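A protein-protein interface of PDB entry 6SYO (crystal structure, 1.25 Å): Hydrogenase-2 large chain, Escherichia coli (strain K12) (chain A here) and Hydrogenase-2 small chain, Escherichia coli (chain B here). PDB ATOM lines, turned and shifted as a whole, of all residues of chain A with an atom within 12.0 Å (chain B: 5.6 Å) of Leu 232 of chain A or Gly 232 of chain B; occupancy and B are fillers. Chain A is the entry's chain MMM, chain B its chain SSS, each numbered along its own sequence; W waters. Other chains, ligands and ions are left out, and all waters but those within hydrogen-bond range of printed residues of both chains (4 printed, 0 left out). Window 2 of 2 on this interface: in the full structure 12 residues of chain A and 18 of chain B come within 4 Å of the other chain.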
ATOM      1  N   ALA A 224      -4.251   1.907  18.715  1.00  0.00           N
ATOM      2  CA  ALA A 224      -4.403   0.477  18.429  1.00  0.00           C
ATOM      3  C   ALA A 224      -4.184   0.127  16.968  1.00  0.00           C
ATOM      4  O   ALA A 224      -4.230  -1.062  16.594  1.00  0.00           O
ATOM      5  CB  ALA A 224      -5.720  -0.040  18.911  1.00  0.00           C
ATOM      6  N   ASN A 225      -4.013   1.121  16.064  1.00  0.00           N
ATOM      7  CA  ASN A 225      -3.765   0.814  14.647  1.00  0.00           C
ATOM      8  C   ASN A 225      -2.378   0.173  14.494  1.00  0.00           C
ATOM      9  O   ASN A 225      -1.391   0.769  15.009  1.00  0.00           O
ATOM     10  CB  ASN A 225      -3.783   2.136  13.844  1.00  0.00           C
ATOM     11  CG  ASN A 225      -5.032   2.982  14.043  1.00  0.00           C
ATOM     12  OD1 ASN A 225      -5.079   3.749  15.049  1.00  0.00           O
ATOM     13  ND2 ASN A 225      -6.061   2.777  13.185  1.00  0.00           N
ATOM     14  N   PRO A 226      -2.243  -0.950  13.772  1.00  0.00           N
ATOM     15  CA  PRO A 226      -0.917  -1.577  13.580  1.00  0.00           C
ATOM     16  C   PRO A 226      -0.323  -1.107  12.251  1.00  0.00           C
ATOM     17  O   PRO A 226      -0.853  -1.479  11.175  1.00  0.00           O
ATOM     18  CB  PRO A 226      -1.234  -3.107  13.579  1.00  0.00           C
ATOM     19  CG  PRO A 226      -2.739  -3.258  13.602  1.00  0.00           C
ATOM     20  CD  PRO A 226      -3.305  -1.863  13.287  1.00  0.00           C
ATOM     21  N   ILE A 227       0.724  -0.274  12.276  1.00  0.00           N
ATOM     22  CA  ILE A 227       1.335   0.235  11.020  1.00  0.00           C
ATOM     23  C   ILE A 227       2.273  -0.819  10.442  1.00  0.00           C
ATOM     24  O   ILE A 227       3.285  -1.183  11.107  1.00  0.00           O
ATOM     25  CB  ILE A 227       2.078   1.575  11.233  1.00  0.00           C
ATOM     26  CG1 ILE A 227       1.083   2.693  11.652  1.00  0.00           C
ATOM     27  CG2 ILE A 227       2.926   1.930  10.025  1.00  0.00           C
ATOM     28  CD1 ILE A 227       1.728   4.009  12.010  1.00  0.00           C
ATOM     29  N   ASN A 228       2.016  -1.294   9.222  1.00  0.00           N
ATOM     30  CA  ASN A 228       2.895  -2.281   8.542  1.00  0.00           C
ATOM     31  C   ASN A 228       2.550  -2.201   7.038  1.00  0.00           C
ATOM     32  O   ASN A 228       1.560  -2.821   6.612  1.00  0.00           O
ATOM     33  CB  ASN A 228       2.709  -3.691   9.111  1.00  0.00           C
ATOM     34  CG  ASN A 228       3.654  -4.708   8.467  1.00  0.00           C
ATOM     35  OD1 ASN A 228       4.397  -4.365   7.516  1.00  0.00           O
ATOM     36  ND2 ASN A 228       3.538  -5.948   8.938  1.00  0.00           N
ATOM     37  N   LEU A 229       3.360  -1.474   6.274  1.00  0.00           N
ATOM     38  CA  LEU A 229       3.060  -1.320   4.829  1.00  0.00           C
ATOM     39  C   LEU A 229       2.965  -2.615   4.099  1.00  0.00           C
ATOM     40  O   LEU A 229       2.255  -2.700   3.039  1.00  0.00           O
ATOM     41  CB  LEU A 229       4.082  -0.428   4.111  1.00  0.00           C
ATOM     42  CG  LEU A 229       4.141   1.021   4.609  1.00  0.00           C
ATOM     43  CD1 LEU A 229       4.952   1.857   3.653  1.00  0.00           C
ATOM     44  CD2 LEU A 229       2.780   1.708   4.799  1.00  0.00           C
ATOM     45  N   ASP A 230       3.658  -3.666   4.579  1.00  0.00           N
ATOM     46  CA  ASP A 230       3.756  -4.994   3.953  1.00  0.00           C
ATOM     47  C   ASP A 230       2.852  -6.050   4.602  1.00  0.00           C
ATOM     48  O   ASP A 230       2.907  -7.245   4.238  1.00  0.00           O
ATOM     49  CB  ASP A 230       5.230  -5.426   3.905  1.00  0.00           C
ATOM     50  CG  ASP A 230       6.030  -4.508   2.987  1.00  0.00           C
ATOM     51  OD1 ASP A 230       5.682  -4.328   1.766  1.00  0.00           O
ATOM     52  OD2 ASP A 230       6.990  -3.824   3.551  1.00  0.00           O
ATOM     53  N   GLY A 231       1.955  -5.643   5.560  1.00  0.00           N
ATOM     54  CA  GLY A 231       1.114  -6.583   6.288  1.00  0.00           C
ATOM     55  C   GLY A 231      -0.295  -6.750   5.715  1.00  0.00           C
ATOM     56  O   GLY A 231      -0.929  -5.781   5.319  1.00  0.00           O
ATOM     57  N   LEU A 232      -0.825  -7.966   5.711  1.00  0.00           N
ATOM     58  CA  LEU A 232      -2.217  -8.308   5.370  1.00  0.00           C
ATOM     59  C   LEU A 232      -3.084  -8.053   6.598  1.00  0.00           C
ATOM     60  O   LEU A 232      -2.699  -8.459   7.739  1.00  0.00           O
ATOM     61  CB  LEU A 232      -2.221  -9.766   4.861  1.00  0.00           C
ATOM     62  CG  LEU A 232      -3.562 -10.298   4.317  1.00  0.00           C
ATOM     63  CD1 LEU A 232      -3.300 -11.385   3.263  1.00  0.00           C
ATOM     64  CD2 LEU A 232      -4.443 -10.841   5.404  1.00  0.00           C
ATOM     65  N   GLY A 233      -4.233  -7.389   6.432  1.00  0.00           N
ATOM     66  CA  GLY A 233      -5.174  -7.178   7.541  1.00  0.00           C
ATOM     67  C   GLY A 233      -4.865  -6.070   8.497  1.00  0.00           C
ATOM     68  O   GLY A 233      -5.613  -5.976   9.524  1.00  0.00           O
ATOM     69  N   VAL A 234      -3.854  -5.226   8.237  1.00  0.00           N
ATOM     70  CA  VAL A 234      -3.423  -4.131   9.128  1.00  0.00           C
ATOM     71  C   VAL A 234      -3.344  -2.804   8.355  1.00  0.00           C
ATOM     72  O   VAL A 234      -3.844  -2.741   7.184  1.00  0.00           O
ATOM     73  CB  VAL A 234      -2.111  -4.539   9.827  1.00  0.00           C
ATOM     74  CG1 VAL A 234      -2.257  -5.845  10.660  1.00  0.00           C
ATOM     75  CG2 VAL A 234      -0.940  -4.650   8.862  1.00  0.00           C
ATOM     76  N   LEU A 235      -2.808  -1.754   8.964  1.00  0.00           N
ATOM     77  CA  LEU A 235      -2.759  -0.415   8.329  1.00  0.00           C
ATOM     78  C   LEU A 235      -1.553  -0.383   7.370  1.00  0.00           C
ATOM     79  O   LEU A 235      -0.406  -0.116   7.784  1.00  0.00           O
ATOM     80  CB  LEU A 235      -2.707   0.704   9.383  1.00  0.00           C
ATOM     81  CG  LEU A 235      -2.772   2.153   8.851  1.00  0.00           C
ATOM     82  CD1 LEU A 235      -4.004   2.398   8.022  1.00  0.00           C
ATOM     83  CD2 LEU A 235      -2.730   3.146  10.004  1.00  0.00           C
ATOM     84  N   ASN A 236      -1.843  -0.716   6.104  1.00  0.00           N
ATOM     85  CA  ASN A 236      -0.832  -0.865   5.045  1.00  0.00           C
ATOM     86  C   ASN A 236      -0.974   0.272   4.025  1.00  0.00           C
ATOM     87  O   ASN A 236      -1.752   1.223   4.230  1.00  0.00           O
ATOM     88  CB  ASN A 236      -0.881  -2.282   4.471  1.00  0.00           C
ATOM     89  CG  ASN A 236      -2.217  -2.581   3.814  1.00  0.00           C
ATOM     90  OD1 ASN A 236      -2.889  -1.657   3.308  1.00  0.00           O
ATOM     91  ND2 ASN A 236      -2.606  -3.871   3.705  1.00  0.00           N
ATOM     92  N   LEU A 237      -0.186   0.229   2.942  1.00  0.00           N
ATOM     93  CA  LEU A 237      -0.223   1.365   1.987  1.00  0.00           C
ATOM     94  C   LEU A 237      -1.584   1.437   1.254  1.00  0.00           C
ATOM     95  O   LEU A 237      -2.095   2.552   0.991  1.00  0.00           O
ATOM     96  CB  LEU A 237       0.927   1.300   0.998  1.00  0.00           C
ATOM     97  CG  LEU A 237       1.111   2.546   0.097  1.00  0.00           C
ATOM     98  CD1 LEU A 237       1.307   3.848   0.923  1.00  0.00           C
ATOM     99  CD2 LEU A 237       2.332   2.335  -0.832  1.00  0.00           C
ATOM    100  N   GLU A 238      -2.200   0.303   0.923  1.00  0.00           N
ATOM    101  CA  GLU A 238      -3.540   0.307   0.278  1.00  0.00           C
ATOM    102  C   GLU A 238      -4.586   1.031   1.184  1.00  0.00           C
ATOM    103  O   GLU A 238      -5.400   1.844   0.698  1.00  0.00           O
ATOM    104  CB  GLU A 238      -3.958  -1.150  -0.049  1.00  0.00           C
ATOM    105  CG  GLU A 238      -5.360  -1.266  -0.665  1.00  0.00           C
ATOM    106  CD  GLU A 238      -6.459  -1.291   0.384  1.00  0.00           C
ATOM    107  OE1 GLU A 238      -6.270  -1.866   1.496  1.00  0.00           O
ATOM    108  OE2 GLU A 238      -7.621  -0.828   0.070  1.00  0.00           O
ATOM    109  N   ARG A 239      -4.573   0.721   2.497  1.00  0.00           N
ATOM    110  CA  ARG A 239      -5.537   1.359   3.435  1.00  0.00           C
ATOM    111  C   ARG A 239      -5.254   2.877   3.528  1.00  0.00           C
ATOM    112  O   ARG A 239      -6.225   3.706   3.530  1.00  0.00           O
ATOM    113  CB  ARG A 239      -5.459   0.712   4.819  1.00  0.00           C
ATOM    114  CG  ARG A 239      -5.890  -0.764   4.944  1.00  0.00           C
ATOM    115  CD  ARG A 239      -7.420  -1.029   4.972  1.00  0.00           C
ATOM    116  NE  ARG A 239      -7.988  -1.011   3.637  1.00  0.00           N
ATOM    117  CZ  ARG A 239      -9.315  -1.068   3.402  1.00  0.00           C
ATOM    118  NH1 ARG A 239     -10.183  -1.086   4.414  1.00  0.00           N
ATOM    119  NH2 ARG A 239      -9.742  -1.119   2.129  1.00  0.00           N
ATOM    120  N   LEU A 240      -3.963   3.261   3.573  1.00  0.00           N
ATOM    121  CA  LEU A 240      -3.612   4.705   3.618  1.00  0.00           C
ATOM    122  C   LEU A 240      -4.063   5.425   2.335  1.00  0.00           C
ATOM    123  O   LEU A 240      -4.639   6.544   2.422  1.00  0.00           O
ATOM    124  CB  LEU A 240      -2.086   4.838   3.860  1.00  0.00           C
ATOM    125  CG  LEU A 240      -1.670   4.491   5.284  1.00  0.00           C
ATOM    126  CD1 LEU A 240      -0.162   4.253   5.375  1.00  0.00           C
ATOM    127  CD2 LEU A 240      -2.061   5.575   6.290  1.00  0.00           C
ATOM    128  N   THR B 183       3.575  -9.432  -0.151  1.00  0.00           N
ATOM    129  CA  THR B 183       3.092 -10.028   1.122  1.00  0.00           C
ATOM    130  C   THR B 183       1.815  -9.323   1.635  1.00  0.00           C
ATOM    131  O   THR B 183       1.005 -10.032   2.312  1.00  0.00           O
ATOM    132  CB  THR B 183       4.190 -10.110   2.217  1.00  0.00           C
ATOM    133  OG1 THR B 183       4.638  -8.796   2.580  1.00  0.00           O
ATOM    134  CG2 THR B 183       5.418 -10.903   1.786  1.00  0.00           C
ATOM    135  N   PHE B 184       1.622  -8.048   1.384  1.00  0.00           N
ATOM    136  CA  PHE B 184       0.425  -7.338   1.946  1.00  0.00           C
ATOM    137  C   PHE B 184      -0.851  -7.970   1.379  1.00  0.00           C
ATOM    138  O   PHE B 184      -1.922  -7.825   2.018  1.00  0.00           O
ATOM    139  CB  PHE B 184       0.406  -5.806   1.736  1.00  0.00           C
ATOM    140  CG  PHE B 184       0.047  -5.365   0.335  1.00  0.00           C
ATOM    141  CD1 PHE B 184       1.008  -5.219  -0.680  1.00  0.00           C
ATOM    142  CD2 PHE B 184      -1.297  -5.067   0.015  1.00  0.00           C
ATOM    143  CE1 PHE B 184       0.620  -4.843  -1.965  1.00  0.00           C
ATOM    144  CE2 PHE B 184      -1.650  -4.667  -1.285  1.00  0.00           C
ATOM    145  CZ  PHE B 184      -0.704  -4.549  -2.268  1.00  0.00           C
ATOM    146  N   ALA B 185      -0.777  -8.589   0.191  1.00  0.00           N
ATOM    147  CA  ALA B 185      -1.924  -9.144  -0.519  1.00  0.00           C
ATOM    148  C   ALA B 185      -1.949 -10.683  -0.579  1.00  0.00           C
ATOM    149  O   ALA B 185      -3.065 -11.265  -0.678  1.00  0.00           O
ATOM    150  CB  ALA B 185      -2.013  -8.559  -1.934  1.00  0.00           C
ATOM    151  N   TYR B 186      -0.780 -11.370  -0.553  1.00  0.00           N
ATOM    152  CA  TYR B 186      -0.712 -12.813  -0.815  1.00  0.00           C
ATOM    153  C   TYR B 186       0.030 -13.536   0.304  1.00  0.00           C
ATOM    154  O   TYR B 186       0.351 -14.741   0.130  1.00  0.00           O
ATOM    155  CB  TYR B 186      -0.089 -13.132  -2.184  1.00  0.00           C
ATOM    156  CG  TYR B 186      -0.825 -12.427  -3.342  1.00  0.00           C
ATOM    157  CD1 TYR B 186      -1.985 -12.998  -3.887  1.00  0.00           C
ATOM    158  CD2 TYR B 186      -0.433 -11.158  -3.802  1.00  0.00           C
ATOM    159  CE1 TYR B 186      -2.692 -12.360  -4.910  1.00  0.00           C
ATOM    160  CE2 TYR B 186      -1.125 -10.515  -4.835  1.00  0.00           C
ATOM    161  CZ  TYR B 186      -2.292 -11.089  -5.356  1.00  0.00           C
ATOM    162  OH  TYR B 186      -2.958 -10.397  -6.361  1.00  0.00           O
ATOM    163  N   GLY B 187       0.275 -12.916   1.453  1.00  0.00           N
ATOM    164  CA  GLY B 187       1.138 -13.503   2.495  1.00  0.00           C
ATOM    165  C   GLY B 187       0.511 -14.579   3.360  1.00  0.00           C
ATOM    166  O   GLY B 187       1.248 -15.144   4.204  1.00  0.00           O
ATOM    167  N   ARG B 188      -0.780 -14.882   3.216  1.00  0.00           N
ATOM    168  CA  ARG B 188      -1.540 -15.777   4.092  1.00  0.00           C
ATOM    169  C   ARG B 188      -2.541 -16.619   3.294  1.00  0.00           C
ATOM    170  O   ARG B 188      -3.151 -16.083   2.319  1.00  0.00           O
ATOM    171  CB  ARG B 188      -2.217 -14.978   5.220  1.00  0.00           C
ATOM    172  CG  ARG B 188      -3.038 -15.745   6.267  1.00  0.00           C
ATOM    173  CD  ARG B 188      -3.450 -14.859   7.423  1.00  0.00           C
ATOM    174  NE  ARG B 188      -2.296 -14.460   8.234  1.00  0.00           N
ATOM    175  CZ  ARG B 188      -2.133 -13.324   8.889  1.00  0.00           C
ATOM    176  NH1 ARG B 188      -3.089 -12.410   8.943  1.00  0.00           N
ATOM    177  NH2 ARG B 188      -0.958 -13.055   9.479  1.00  0.00           N
ATOM    178  N   LEU B 189      -2.810 -17.867   3.686  1.00  0.00           N
ATOM    179  CA  LEU B 189      -3.894 -18.651   3.125  1.00  0.00           C
ATOM    180  C   LEU B 189      -5.231 -17.991   3.405  1.00  0.00           C
ATOM    181  O   LEU B 189      -5.474 -17.468   4.522  1.00  0.00           O
ATOM    182  CB  LEU B 189      -3.882 -20.064   3.708  1.00  0.00           C
ATOM    183  CG  LEU B 189      -2.706 -20.984   3.274  1.00  0.00           C
ATOM    184  CD1 LEU B 189      -2.650 -22.227   4.197  1.00  0.00           C
ATOM    185  CD2 LEU B 189      -2.861 -21.398   1.821  1.00  0.00           C
ATOM    186  N   ILE B 190      -6.185 -18.035   2.471  1.00  0.00           N
ATOM    187  CA  ILE B 190      -7.568 -17.530   2.689  1.00  0.00           C
ATOM    188  C   ILE B 190      -8.165 -18.235   3.918  1.00  0.00           C
ATOM    189  O   ILE B 190      -8.769 -17.534   4.809  1.00  0.00           O
ATOM    190  CB  ILE B 190      -8.431 -17.647   1.411  1.00  0.00           C
ATOM    191  CG1 ILE B 190      -7.906 -16.650   0.340  1.00  0.00           C
ATOM    192  CG2 ILE B 190      -9.901 -17.428   1.712  1.00  0.00           C
ATOM    193  CD1 ILE B 190      -8.481 -16.928  -1.060  1.00  0.00           C
ATOM    194  N   HIS B 193      -7.514 -16.875   7.421  1.00  0.00           N
ATOM    195  CA  HIS B 193      -8.095 -15.542   7.770  1.00  0.00           C
ATOM    196  C   HIS B 193      -9.548 -15.465   7.284  1.00  0.00           C
ATOM    197  O   HIS B 193      -9.973 -14.393   6.831  1.00  0.00           O
ATOM    198  CB  HIS B 193      -7.212 -14.358   7.328  1.00  0.00           C
ATOM    199  CG  HIS B 193      -7.216 -13.159   8.226  1.00  0.00           C
ATOM    200  ND1 HIS B 193      -6.115 -12.814   9.008  1.00  0.00           N
ATOM    201  CD2 HIS B 193      -8.223 -12.268   8.480  1.00  0.00           C
ATOM    202  CE1 HIS B 193      -6.469 -11.720   9.717  1.00  0.00           C
ATOM    203  NE2 HIS B 193      -7.779 -11.359   9.406  1.00  0.00           N
ATOM    204  N   THR B 230      -5.111 -21.888  -1.027  1.00  0.00           N
ATOM    205  CA  THR B 230      -4.995 -20.655  -1.898  1.00  0.00           C
ATOM    206  C   THR B 230      -4.472 -19.472  -1.078  1.00  0.00           C
ATOM    207  O   THR B 230      -5.153 -19.111  -0.074  1.00  0.00           O
ATOM    208  CB  THR B 230      -6.384 -20.353  -2.543  1.00  0.00           C
ATOM    209  OG1 THR B 230      -6.826 -21.525  -3.259  1.00  0.00           O
ATOM    210  CG2 THR B 230      -6.266 -19.204  -3.504  1.00  0.00           C
ATOM    211  N   TYR B 231      -3.390 -18.837  -1.468  1.00  0.00           N
ATOM    212  CA  TYR B 231      -2.879 -17.612  -0.814  1.00  0.00           C
ATOM    213  C   TYR B 231      -3.581 -16.391  -1.451  1.00  0.00           C
ATOM    214  O   TYR B 231      -3.739 -16.328  -2.690  1.00  0.00           O
ATOM    215  CB  TYR B 231      -1.355 -17.485  -1.015  1.00  0.00           C
ATOM    216  CG  TYR B 231      -0.572 -18.469  -0.135  1.00  0.00           C
ATOM    217  CD1 TYR B 231      -0.268 -19.758  -0.575  1.00  0.00           C
ATOM    218  CD2 TYR B 231      -0.209 -18.089   1.147  1.00  0.00           C
ATOM    219  CE1 TYR B 231       0.391 -20.643   0.296  1.00  0.00           C
ATOM    220  CE2 TYR B 231       0.419 -18.986   2.020  1.00  0.00           C
ATOM    221  CZ  TYR B 231       0.706 -20.265   1.588  1.00  0.00           C
ATOM    222  OH  TYR B 231       1.376 -21.125   2.456  1.00  0.00           O
ATOM    223  N   GLY B 232      -4.011 -15.430  -0.624  1.00  0.00           N
ATOM    224  CA  GLY B 232      -4.726 -14.228  -1.137  1.00  0.00           C
ATOM    225  C   GLY B 232      -5.309 -13.408  -0.014  1.00  0.00           C
ATOM    226  O   GLY B 232      -5.172 -13.732   1.178  1.00  0.00           O
ATOM    227  N   ASN B 233      -5.973 -12.320  -0.385  1.00  0.00           N
ATOM    228  CA  ASN B 233      -6.596 -11.365   0.557  1.00  0.00           C
ATOM    229  C   ASN B 233      -8.109 -11.245   0.306  1.00  0.00           C
ATOM    230  O   ASN B 233      -8.751 -10.253   0.720  1.00  0.00           O
ATOM    231  CB  ASN B 233      -5.898  -9.981   0.561  1.00  0.00           C
ATOM    232  CG  ASN B 233      -5.972  -9.237  -0.766  1.00  0.00           C
ATOM    233  OD1 ASN B 233      -6.559  -9.739  -1.761  1.00  0.00           O
ATOM    234  ND2 ASN B 233      -5.327  -8.039  -0.814  1.00  0.00           N
ATOM    235  N   CYS B 234      -8.719 -12.250  -0.307  1.00  0.00           N
ATOM    236  CA  CYS B 234     -10.122 -12.146  -0.728  1.00  0.00           C
ATOM    237  C   CYS B 234     -11.072 -12.028   0.447  1.00  0.00           C
ATOM    238  O   CYS B 234     -12.134 -11.368   0.303  1.00  0.00           O
ATOM    239  CB  CYS B 234     -10.505 -13.343  -1.590  1.00  0.00           C
ATOM    240  SG  CYS B 234      -9.442 -13.493  -3.071  1.00  0.00           S
ATOM    241  N   THR B 236     -10.447 -10.448   3.366  1.00  0.00           N
ATOM    242  CA  THR B 236     -10.180  -9.226   4.146  1.00  0.00           C
ATOM    243  C   THR B 236     -10.353  -8.002   3.234  1.00  0.00           C
ATOM    244  O   THR B 236     -11.292  -7.196   3.479  1.00  0.00           O
ATOM    245  CB  THR B 236      -8.799  -9.267   4.823  1.00  0.00           C
ATOM    246  OG1 THR B 236      -7.798  -9.631   3.864  1.00  0.00           O
ATOM    247  CG2 THR B 236      -8.763 -10.175   6.038  1.00  0.00           C
ATOM    248  N   ASN B 258      -6.316 -17.801  -7.762  1.00  0.00           N
ATOM    249  CA  ASN B 258      -5.009 -17.194  -7.511  1.00  0.00           C
ATOM    250  C   ASN B 258      -3.857 -18.189  -7.735  1.00  0.00           C
ATOM    251  O   ASN B 258      -2.692 -17.716  -7.958  1.00  0.00           O
ATOM    252  CB  ASN B 258      -4.844 -16.650  -6.080  1.00  0.00           C
ATOM    253  CG  ASN B 258      -5.533 -15.321  -5.802  1.00  0.00           C
ATOM    254  OD1 ASN B 258      -6.224 -14.769  -6.690  1.00  0.00           O
ATOM    255  ND2 ASN B 258      -5.321 -14.803  -4.568  1.00  0.00           N
HETATM  256  O   HOH W   1       4.054  -6.329   0.570  1.00  0.00           O
HETATM  257  O   HOH W   2       1.380 -10.478   5.103  1.00  0.00           O
HETATM  258  O   HOH W   3      -5.989  -7.459   3.971  1.00  0.00           O
HETATM  259  O   HOH W   4      -9.995  -4.517   4.308  1.00  0.00           O
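The side-chain hydroxyl of Thr 183 of chain B is in hydrogen-bond range of the backbone carbonyl oxygen of Asp 230 of chain A, at 2.9 Å.
The backbone carbonyl oxygen (O) of Asp 230 of chain A is in hydrogen-bond range of the backbone NH (N) of Phe 184 of chain B (3.2 Å).
The backbone NH of Asn 233 of chain B is in hydrogen-bond range of the backbone carbonyl oxygen of Ala 185 of chain B (3.1 Å).
The backbone NH (N) of Gly 232 of chain B sits at hydrogen-bond distance from the backbone carbonyl oxygen (O) of Arg 188 of chain B, 3.1 Å away.
O of Asn 233 of chain B lies within hydrogen-bond range of OG1 of Thr 236 of chain B, at 3.3 Å.
The backbone NH of Asp 230 of chain A sits close to the side-chain amide oxygen of Asn 228 of chain A, at 3.1 Å.
The side-chain amide oxygen (OD1) of Asn 228 of chain A lies within hydrogen-bond range of the backbone NH (N) of Gly 231 of chain A, at 3.4 Å.
ND2 of Asn 236 of chain A lies within hydrogen-bond range of O of Gly 231 of chain A, 3.0 Å away.
Among the printed residues, merely in contact across the chains: Leu 232 of chain A with Phe 184 of chain B, Leu 232 of chain A with Gly 232 of chain B, Gly 231 of chain A with Phe 184 of chain B, Leu 229 of chain A with Phe 184 of chain B, Leu 232 of chain A with Thr 236 of chain B and Leu 232 of chain A with Ala 185 of chain B.
Printed residues of chain B within 4 Å of Leu 232 of chain A: Phe 184, Ala 185, Gly 232 and Thr 236.
Gly 232 of chain B touches one residue of chain A.
Thr 183 of chain B touches just one residue of chain A: Asp 230.
Of chain A, only Leu 232 comes within 4 Å of Ala 185 of chain B.
No residue of chain A comes within 4 Å of Gly 187 of chain B.
Cys 234 of chain B touches none of the printed residues of chain A.
Printed residues of chain B within 4 Å of Gly 231 of chain A: Phe 184.
Of the printed residues of chain A, Thr 236 of chain B touches Leu 232 (3.9 Å).
Leu 237 of chain A touches none of the printed residues of chain B.
The nearest printed residue of chain B that does not touch Leu 232 of chain A is Asn 233 of chain B (4.003 Å).
Hydrophobic or aromatic side chains of chain B within 4 Å of the printed part of chain A: Phe 184.
Among the printed residues, 8 pairs touch across the chains.
Among the printed residues, no Asp or Glu carboxylate lies within 4 Å of a Lys or Arg side-chain nitrogen of the other chain.
Water W3 bridges the side-chain hydroxyl of Thr 236 of chain B (2.8 Å) and the backbone NH of Gly 233 of chain A (3.0 Å).
Water W1 lies within hydrogen-bond range of OD1 of Asp 230 of chain A (2.8 Å), N of Phe 184 of chain B (3.1 Å) and N of Thr 183 of chain B (3.2 Å).
Water W2 lies within hydrogen-bond range of the backbone carbonyl oxygen (O) of Thr 183 of chain B and the backbone NH (N) of Leu 232 of chain A.
Water W4 lies within hydrogen-bond range of O of Thr 236 of chain B (3.1 Å) and NH1 of Arg 239 of chain A (3.4 Å).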
